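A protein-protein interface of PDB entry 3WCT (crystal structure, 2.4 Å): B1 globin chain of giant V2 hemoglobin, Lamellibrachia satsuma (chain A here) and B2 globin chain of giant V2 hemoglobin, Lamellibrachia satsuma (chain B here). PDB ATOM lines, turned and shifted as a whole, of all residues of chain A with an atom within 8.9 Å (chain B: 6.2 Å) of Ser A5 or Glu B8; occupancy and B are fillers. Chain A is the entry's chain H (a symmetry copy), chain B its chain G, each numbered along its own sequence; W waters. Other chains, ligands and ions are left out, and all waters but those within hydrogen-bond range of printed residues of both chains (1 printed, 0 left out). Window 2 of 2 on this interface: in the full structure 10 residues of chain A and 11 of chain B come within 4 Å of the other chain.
N of Asp A8 is in hydrogen-bond range of OG of Ser A5 (3.3 Å).
The side-chain sulfur (SG) of Cys A136 forms a disulfide with the side-chain sulfur (SG) of Cys A4, 2.0 Å away.
The side-chain amide nitrogen (ND2) of Asn A135 sits at hydrogen-bond distance from the side-chain carboxylate (OD1) of Asp A8, at 2.7 Å.
O of Asp A131 lies close to ND2 of Asn A135, 3.4 Å away.
OE2 of Glu B8 lies within hydrogen-bond range of OG1 of Thr B6.
OD2 of Asp B9 sits at hydrogen-bond distance from OG1 of Thr B6, at 3.1 Å.
Phe A3 touches none of the printed residues of chain B.
Of chain B, only Thr B6 (3.7 Å) and Glu B8 (2.5 Å) come within 4 Å of Ser A5.
Of the printed residues of chain B, Ala A7 touches Thr B7 and Glu B8.
Printed residues of chain B within 4 Å of Ile A11: Thr B7.
Asn A83 touches none of the printed residues of chain B.
Of the printed residues of chain B, Asp A131 touches Arg B10.
Printed residues of chain B within 4 Å of Asn A135: Thr B6 (3.9 Å).
Printed residues of chain A within 4 Å of Thr B6: Ser A5, Asp A8 and Asn A135.
Of chain A, only Ala A7, Asp A8 and Ile A11 come within 4 Å of Thr B7.
Glu B8 touches two residues of chain A.
Of the 9 printed residues of chain B, 4 touch a printed residue of chain A.
Among the printed residues, 9 pairs touch across the chains.
Among the printed residues, merely in contact across the chains: Asp A8 with Thr B6, Ile A11 with Thr B7, Ala A7 with Thr B7, Ser A5 with Thr B6 and Asn A135 with Thr B6.
Water W1 bridges the side-chain amide oxygen (OD1) of Asn A135 (3.1 Å) and the guanidinium group (NH2) of Arg B10 (3.2 Å).
The side-chain carboxylate (OE2) of Glu B8 is in hydrogen-bond range of the side-chain hydroxyl (OG) of Ser A5 (2.5 Å).
The guanidinium group of Arg B10 is in salt-bridge range of the side-chain carboxylate of Asp A131 (2.9 Å).
N of Thr B7 sits at hydrogen-bond distance from OD2 of Asp A8 (2.9 Å).
N of Ala A7 sits close to OE1 of Glu B8.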
ATOM      1  N   PHE A   3     -16.158  -0.239 -16.014  1.00  0.00           N
ATOM      2  CA  PHE A   3     -17.235  -1.210 -16.184  1.00  0.00           C
ATOM      3  C   PHE A   3     -18.540  -0.691 -15.590  1.00  0.00           C
ATOM      4  O   PHE A   3     -19.293   0.019 -16.266  1.00  0.00           O
ATOM      5  CB  PHE A   3     -16.838  -2.535 -15.531  1.00  0.00           C
ATOM      6  CG  PHE A   3     -15.678  -3.207 -16.204  1.00  0.00           C
ATOM      7  CD1 PHE A   3     -15.876  -3.997 -17.329  1.00  0.00           C
ATOM      8  CD2 PHE A   3     -14.379  -2.992 -15.759  1.00  0.00           C
ATOM      9  CE1 PHE A   3     -14.795  -4.560 -18.005  1.00  0.00           C
ATOM     10  CE2 PHE A   3     -13.294  -3.549 -16.429  1.00  0.00           C
ATOM     11  CZ  PHE A   3     -13.504  -4.334 -17.556  1.00  0.00           C
ATOM     12  N   CYS A   4     -18.808  -1.049 -14.334  1.00  0.00           N
ATOM     13  CA  CYS A   4     -20.014  -0.601 -13.647  1.00  0.00           C
ATOM     14  C   CYS A   4     -19.664  -0.129 -12.231  1.00  0.00           C
ATOM     15  O   CYS A   4     -18.542  -0.329 -11.766  1.00  0.00           O
ATOM     16  CB  CYS A   4     -21.073  -1.723 -13.623  1.00  0.00           C
ATOM     17  SG  CYS A   4     -20.630  -3.278 -12.779  1.00  0.00           S
ATOM     18  N   SER A   5     -20.609   0.512 -11.551  1.00  0.00           N
ATOM     19  CA  SER A   5     -20.348   1.027 -10.207  1.00  0.00           C
ATOM     20  C   SER A   5     -20.223  -0.062  -9.154  1.00  0.00           C
ATOM     21  O   SER A   5     -20.636  -1.199  -9.366  1.00  0.00           O
ATOM     22  CB  SER A   5     -21.452   1.998  -9.783  1.00  0.00           C
ATOM     23  OG  SER A   5     -22.623   1.297  -9.414  1.00  0.00           O
ATOM     24  N   GLU A   6     -19.652   0.304  -8.014  1.00  0.00           N
ATOM     25  CA  GLU A   6     -19.458  -0.617  -6.905  1.00  0.00           C
ATOM     26  C   GLU A   6     -20.766  -1.193  -6.362  1.00  0.00           C
ATOM     27  O   GLU A   6     -20.816  -2.366  -5.982  1.00  0.00           O
ATOM     28  CB  GLU A   6     -18.694   0.079  -5.768  1.00  0.00           C
ATOM     29  CG  GLU A   6     -18.581  -0.751  -4.484  1.00  0.00           C
ATOM     30  CD  GLU A   6     -17.691  -0.101  -3.435  1.00  0.00           C
ATOM     31  OE1 GLU A   6     -16.450  -0.256  -3.512  1.00  0.00           O
ATOM     32  OE2 GLU A   6     -18.230   0.576  -2.530  1.00  0.00           O
ATOM     33  N   ALA A   7     -21.812  -0.372  -6.321  1.00  0.00           N
ATOM     34  CA  ALA A   7     -23.118  -0.799  -5.808  1.00  0.00           C
ATOM     35  C   ALA A   7     -23.841  -1.740  -6.786  1.00  0.00           C
ATOM     36  O   ALA A   7     -24.545  -2.666  -6.370  1.00  0.00           O
ATOM     37  CB  ALA A   7     -23.982   0.417  -5.508  1.00  0.00           C
ATOM     38  N   ASP A   8     -23.663  -1.491  -8.080  1.00  0.00           N
ATOM     39  CA  ASP A   8     -24.261  -2.330  -9.117  1.00  0.00           C
ATOM     40  C   ASP A   8     -23.510  -3.662  -9.163  1.00  0.00           C
ATOM     41  O   ASP A   8     -24.104  -4.740  -9.245  1.00  0.00           O
ATOM     42  CB  ASP A   8     -24.152  -1.647 -10.478  1.00  0.00           C
ATOM     43  CG  ASP A   8     -25.217  -0.592 -10.691  1.00  0.00           C
ATOM     44  OD1 ASP A   8     -25.115   0.156 -11.688  1.00  0.00           O
ATOM     45  OD2 ASP A   8     -26.159  -0.518  -9.874  1.00  0.00           O
ATOM     46  N   ALA A   9     -22.191  -3.573  -9.107  1.00  0.00           N
ATOM     47  CA  ALA A   9     -21.355  -4.757  -9.138  1.00  0.00           C
ATOM     48  C   ALA A   9     -21.718  -5.696  -7.992  1.00  0.00           C
ATOM     49  O   ALA A   9     -21.802  -6.916  -8.174  1.00  0.00           O
ATOM     50  CB  ALA A   9     -19.902  -4.351  -9.036  1.00  0.00           C
ATOM     51  N   THR A  10     -21.940  -5.119  -6.813  1.00  0.00           N
ATOM     52  CA  THR A  10     -22.266  -5.904  -5.634  1.00  0.00           C
ATOM     53  C   THR A  10     -23.552  -6.703  -5.804  1.00  0.00           C
ATOM     54  O   THR A  10     -23.623  -7.868  -5.409  1.00  0.00           O
ATOM     55  CB  THR A  10     -22.379  -5.005  -4.389  1.00  0.00           C
ATOM     56  OG1 THR A  10     -21.109  -4.399  -4.136  1.00  0.00           O
ATOM     57  CG2 THR A  10     -22.799  -5.820  -3.154  1.00  0.00           C
ATOM     58  N   ILE A  11     -24.569  -6.075  -6.384  1.00  0.00           N
ATOM     59  CA  ILE A  11     -25.837  -6.753  -6.608  1.00  0.00           C
ATOM     60  C   ILE A  11     -25.622  -7.927  -7.568  1.00  0.00           C
ATOM     61  O   ILE A  11     -26.045  -9.043  -7.283  1.00  0.00           O
ATOM     62  CB  ILE A  11     -26.889  -5.758  -7.151  1.00  0.00           C
ATOM     63  CG1 ILE A  11     -27.292  -4.798  -6.029  1.00  0.00           C
ATOM     64  CG2 ILE A  11     -28.106  -6.483  -7.651  1.00  0.00           C
ATOM     65  CD1 ILE A  11     -28.144  -3.632  -6.482  1.00  0.00           C
ATOM     66  N   VAL A  12     -24.940  -7.678  -8.682  1.00  0.00           N
ATOM     67  CA  VAL A  12     -24.665  -8.719  -9.666  1.00  0.00           C
ATOM     68  C   VAL A  12     -23.899  -9.897  -9.064  1.00  0.00           C
ATOM     69  O   VAL A  12     -24.281 -11.058  -9.232  1.00  0.00           O
ATOM     70  CB  VAL A  12     -23.860  -8.153 -10.865  1.00  0.00           C
ATOM     71  CG1 VAL A  12     -23.479  -9.273 -11.817  1.00  0.00           C
ATOM     72  CG2 VAL A  12     -24.701  -7.110 -11.611  1.00  0.00           C
ATOM     73  N   ILE A  13     -22.817  -9.593  -8.360  1.00  0.00           N
ATOM     74  CA  ILE A  13     -22.005 -10.617  -7.723  1.00  0.00           C
ATOM     75  C   ILE A  13     -22.831 -11.448  -6.754  1.00  0.00           C
ATOM     76  O   ILE A  13     -22.762 -12.672  -6.759  1.00  0.00           O
ATOM     77  CB  ILE A  13     -20.832  -9.984  -6.955  1.00  0.00           C
ATOM     78  CG1 ILE A  13     -19.810  -9.438  -7.952  1.00  0.00           C
ATOM     79  CG2 ILE A  13     -20.183 -11.024  -6.022  1.00  0.00           C
ATOM     80  CD1 ILE A  13     -18.772  -8.540  -7.319  1.00  0.00           C
ATOM     81  N   LEU A  82     -15.646  -7.580 -11.032  1.00  0.00           N
ATOM     82  CA  LEU A  82     -16.292  -6.330 -11.420  1.00  0.00           C
ATOM     83  C   LEU A  82     -15.809  -5.138 -10.593  1.00  0.00           C
ATOM     84  O   LEU A  82     -15.884  -3.995 -11.044  1.00  0.00           O
ATOM     85  CB  LEU A  82     -17.817  -6.460 -11.301  1.00  0.00           C
ATOM     86  CG  LEU A  82     -18.450  -7.211 -12.477  1.00  0.00           C
ATOM     87  CD1 LEU A  82     -19.932  -7.439 -12.223  1.00  0.00           C
ATOM     88  CD2 LEU A  82     -18.219  -6.405 -13.768  1.00  0.00           C
ATOM     89  N   ASN A  83     -15.315  -5.390  -9.384  1.00  0.00           N
ATOM     90  CA  ASN A  83     -14.820  -4.291  -8.562  1.00  0.00           C
ATOM     91  C   ASN A  83     -13.300  -4.206  -8.515  1.00  0.00           C
ATOM     92  O   ASN A  83     -12.722  -3.674  -7.568  1.00  0.00           O
ATOM     93  CB  ASN A  83     -15.403  -4.356  -7.143  1.00  0.00           C
ATOM     94  CG  ASN A  83     -16.835  -3.816  -7.076  1.00  0.00           C
ATOM     95  OD1 ASN A  83     -17.104  -2.670  -7.464  1.00  0.00           O
ATOM     96  ND2 ASN A  83     -17.756  -4.639  -6.584  1.00  0.00           N
ATOM     97  N   ASP A  84     -12.659  -4.732  -9.552  1.00  0.00           N
ATOM     98  CA  ASP A  84     -11.203  -4.681  -9.692  1.00  0.00           C
ATOM     99  C   ASP A  84     -10.933  -4.448 -11.177  1.00  0.00           C
ATOM    100  O   ASP A  84     -10.360  -5.310 -11.854  1.00  0.00           O
ATOM    101  CB  ASP A  84     -10.557  -5.996  -9.259  1.00  0.00           C
ATOM    102  CG  ASP A  84      -9.037  -5.925  -9.259  1.00  0.00           C
ATOM    103  OD1 ASP A  84      -8.456  -5.314 -10.186  1.00  0.00           O
ATOM    104  OD2 ASP A  84      -8.416  -6.491  -8.333  1.00  0.00           O
ATOM    105  N   ASP A 131     -31.600  -3.971 -14.295  1.00  0.00           N
ATOM    106  CA  ASP A 131     -30.805  -2.754 -14.486  1.00  0.00           C
ATOM    107  C   ASP A 131     -29.362  -2.901 -13.997  1.00  0.00           C
ATOM    108  O   ASP A 131     -28.428  -2.506 -14.699  1.00  0.00           O
ATOM    109  CB  ASP A 131     -31.481  -1.554 -13.812  1.00  0.00           C
ATOM    110  CG  ASP A 131     -32.700  -1.068 -14.580  1.00  0.00           C
ATOM    111  OD1 ASP A 131     -33.320  -0.058 -14.169  1.00  0.00           O
ATOM    112  OD2 ASP A 131     -33.045  -1.691 -15.606  1.00  0.00           O
ATOM    113  N   ALA A 132     -29.168  -3.454 -12.801  1.00  0.00           N
ATOM    114  CA  ALA A 132     -27.808  -3.664 -12.294  1.00  0.00           C
ATOM    115  C   ALA A 132     -27.091  -4.595 -13.268  1.00  0.00           C
ATOM    116  O   ALA A 132     -25.974  -4.313 -13.686  1.00  0.00           O
ATOM    117  CB  ALA A 132     -27.828  -4.295 -10.909  1.00  0.00           C
ATOM    118  N   ASN A 135     -26.203  -2.860 -16.458  1.00  0.00           N
ATOM    119  CA  ASN A 135     -25.099  -1.938 -16.209  1.00  0.00           C
ATOM    120  C   ASN A 135     -23.729  -2.620 -16.191  1.00  0.00           C
ATOM    121  O   ASN A 135     -22.748  -2.047 -16.659  1.00  0.00           O
ATOM    122  CB  ASN A 135     -25.295  -1.178 -14.883  1.00  0.00           C
ATOM    123  CG  ASN A 135     -26.393  -0.116 -14.953  1.00  0.00           C
ATOM    124  OD1 ASN A 135     -26.790   0.311 -16.027  1.00  0.00           O
ATOM    125  ND2 ASN A 135     -26.866   0.325 -13.792  1.00  0.00           N
ATOM    126  N   CYS A 136     -23.661  -3.829 -15.649  1.00  0.00           N
ATOM    127  CA  CYS A 136     -22.394  -4.564 -15.555  1.00  0.00           C
ATOM    128  C   CYS A 136     -22.097  -5.532 -16.694  1.00  0.00           C
ATOM    129  O   CYS A 136     -20.944  -5.675 -17.094  1.00  0.00           O
ATOM    130  CB  CYS A 136     -22.321  -5.335 -14.236  1.00  0.00           C
ATOM    131  SG  CYS A 136     -22.382  -4.298 -12.742  1.00  0.00           S
ATOM    132  N   PRO A 139     -20.878  -3.681 -20.500  1.00  0.00           N
ATOM    133  CA  PRO A 139     -19.448  -3.402 -20.654  1.00  0.00           C
ATOM    134  C   PRO A 139     -18.594  -4.671 -20.710  1.00  0.00           C
ATOM    135  O   PRO A 139     -17.613  -4.744 -21.454  1.00  0.00           O
ATOM    136  CB  PRO A 139     -19.129  -2.554 -19.426  1.00  0.00           C
ATOM    137  CG  PRO A 139     -20.437  -1.861 -19.137  1.00  0.00           C
ATOM    138  CD  PRO A 139     -21.425  -2.983 -19.325  1.00  0.00           C
ATOM    139  N   THR B   6     -27.125   4.296 -12.146  1.00  0.00           N
ATOM    140  CA  THR B   6     -26.580   3.276 -11.247  1.00  0.00           C
ATOM    141  C   THR B   6     -27.323   3.192  -9.921  1.00  0.00           C
ATOM    142  O   THR B   6     -28.125   4.073  -9.579  1.00  0.00           O
ATOM    143  CB  THR B   6     -25.097   3.548 -10.889  1.00  0.00           C
ATOM    144  OG1 THR B   6     -25.032   4.650  -9.974  1.00  0.00           O
ATOM    145  CG2 THR B   6     -24.278   3.866 -12.141  1.00  0.00           C
ATOM    146  N   THR B   7     -27.010   2.137  -9.165  1.00  0.00           N
ATOM    147  CA  THR B   7     -27.621   1.907  -7.869  1.00  0.00           C
ATOM    148  C   THR B   7     -27.435   3.079  -6.924  1.00  0.00           C
ATOM    149  O   THR B   7     -28.358   3.420  -6.184  1.00  0.00           O
ATOM    150  CB  THR B   7     -27.063   0.651  -7.189  1.00  0.00           C
ATOM    151  OG1 THR B   7     -27.508  -0.507  -7.894  1.00  0.00           O
ATOM    152  CG2 THR B   7     -27.558   0.568  -5.752  1.00  0.00           C
ATOM    153  N   GLU B   8     -26.258   3.699  -6.926  1.00  0.00           N
ATOM    154  CA  GLU B   8     -26.073   4.829  -6.028  1.00  0.00           C
ATOM    155  C   GLU B   8     -26.778   6.087  -6.539  1.00  0.00           C
ATOM    156  O   GLU B   8     -27.157   6.943  -5.739  1.00  0.00           O
ATOM    157  CB  GLU B   8     -24.579   5.111  -5.733  1.00  0.00           C
ATOM    158  CG  GLU B   8     -23.603   4.805  -6.843  1.00  0.00           C
ATOM    159  CD  GLU B   8     -23.216   3.343  -6.890  1.00  0.00           C
ATOM    160  OE1 GLU B   8     -22.267   2.931  -6.187  1.00  0.00           O
ATOM    161  OE2 GLU B   8     -23.874   2.602  -7.631  1.00  0.00           O
ATOM    162  N   ASP B   9     -26.977   6.200  -7.851  1.00  0.00           N
ATOM    163  CA  ASP B   9     -27.673   7.366  -8.387  1.00  0.00           C
ATOM    164  C   ASP B   9     -29.141   7.252  -8.019  1.00  0.00           C
ATOM    165  O   ASP B   9     -29.807   8.258  -7.765  1.00  0.00           O
ATOM    166  CB  ASP B   9     -27.575   7.451  -9.912  1.00  0.00           C
ATOM    167  CG  ASP B   9     -26.158   7.652 -10.409  1.00  0.00           C
ATOM    168  OD1 ASP B   9     -25.334   8.240  -9.673  1.00  0.00           O
ATOM    169  OD2 ASP B   9     -25.878   7.232 -11.557  1.00  0.00           O
ATOM    170  N   ARG B  10     -29.645   6.022  -8.010  1.00  0.00           N
ATOM    171  CA  ARG B  10     -31.046   5.774  -7.680  1.00  0.00           C
ATOM    172  C   ARG B  10     -31.332   6.186  -6.241  1.00  0.00           C
ATOM    173  O   ARG B  10     -32.317   6.863  -5.969  1.00  0.00           O
ATOM    174  CB  ARG B  10     -31.392   4.291  -7.889  1.00  0.00           C
ATOM    175  CG  ARG B  10     -31.464   3.883  -9.356  1.00  0.00           C
ATOM    176  CD  ARG B  10     -31.125   2.399  -9.563  1.00  0.00           C
ATOM    177  NE  ARG B  10     -30.724   2.144 -10.949  1.00  0.00           N
ATOM    178  CZ  ARG B  10     -31.536   1.710 -11.905  1.00  0.00           C
ATOM    179  NH1 ARG B  10     -32.809   1.459 -11.644  1.00  0.00           N
ATOM    180  NH2 ARG B  10     -31.080   1.551 -13.133  1.00  0.00           N
ATOM    181  N   ARG B  11     -30.470   5.766  -5.324  1.00  0.00           N
ATOM    182  CA  ARG B  11     -30.638   6.112  -3.926  1.00  0.00           C
ATOM    183  C   ARG B  11     -30.703   7.623  -3.808  1.00  0.00           C
ATOM    184  O   ARG B  11     -31.624   8.163  -3.194  1.00  0.00           O
ATOM    185  CB  ARG B  11     -29.460   5.595  -3.109  1.00  0.00           C
ATOM    186  CG  ARG B  11     -29.345   4.086  -3.084  1.00  0.00           C
ATOM    187  CD  ARG B  11     -27.955   3.663  -2.647  1.00  0.00           C
ATOM    188  NE  ARG B  11     -27.837   2.216  -2.512  1.00  0.00           N
ATOM    189  CZ  ARG B  11     -26.686   1.576  -2.337  1.00  0.00           C
ATOM    190  NH1 ARG B  11     -25.548   2.257  -2.281  1.00  0.00           N
ATOM    191  NH2 ARG B  11     -26.672   0.254  -2.215  1.00  0.00           N
ATOM    192  N   GLU B  12     -29.731   8.292  -4.425  1.00  0.00           N
ATOM    193  CA  GLU B  12     -29.650   9.744  -4.386  1.00  0.00           C
ATOM    194  C   GLU B  12     -30.863  10.437  -5.000  1.00  0.00           C
ATOM    195  O   GLU B  12     -31.274  11.498  -4.529  1.00  0.00           O
ATOM    196  CB  GLU B  12     -28.364  10.224  -5.076  1.00  0.00           C
ATOM    197  CG  GLU B  12     -28.099  11.708  -4.886  1.00  0.00           C
ATOM    198  CD  GLU B  12     -26.680  12.128  -5.262  1.00  0.00           C
ATOM    199  OE1 GLU B  12     -26.360  13.326  -5.080  1.00  0.00           O
ATOM    200  OE2 GLU B  12     -25.889  11.275  -5.735  1.00  0.00           O
ATOM    201  N   MET B  13     -31.439   9.855  -6.045  1.00  0.00           N
ATOM    202  CA  MET B  13     -32.613  10.468  -6.652  1.00  0.00           C
ATOM    203  C   MET B  13     -33.780  10.268  -5.698  1.00  0.00           C
ATOM    204  O   MET B  13     -34.631  11.141  -5.537  1.00  0.00           O
ATOM    205  CB  MET B  13     -32.935   9.833  -8.003  1.00  0.00           C
ATOM    206  CG  MET B  13     -34.094  10.521  -8.711  1.00  0.00           C
ATOM    207  SD  MET B  13     -34.451   9.783 -10.292  1.00  0.00           S
ATOM    208  CE  MET B  13     -35.232  11.144 -11.146  1.00  0.00           C
ATOM    209  N   ALA B 132     -26.842  12.962 -11.619  1.00  0.00           N
ATOM    210  CA  ALA B 132     -27.467  11.750 -11.119  1.00  0.00           C
ATOM    211  C   ALA B 132     -28.953  11.769 -11.436  1.00  0.00           C
ATOM    212  O   ALA B 132     -29.515  10.780 -11.904  1.00  0.00           O
ATOM    213  CB  ALA B 132     -27.255  11.622  -9.587  1.00  0.00           C
HETATM  214  O   HOH W   1     -29.870   0.718 -15.933  1.00  0.00           O
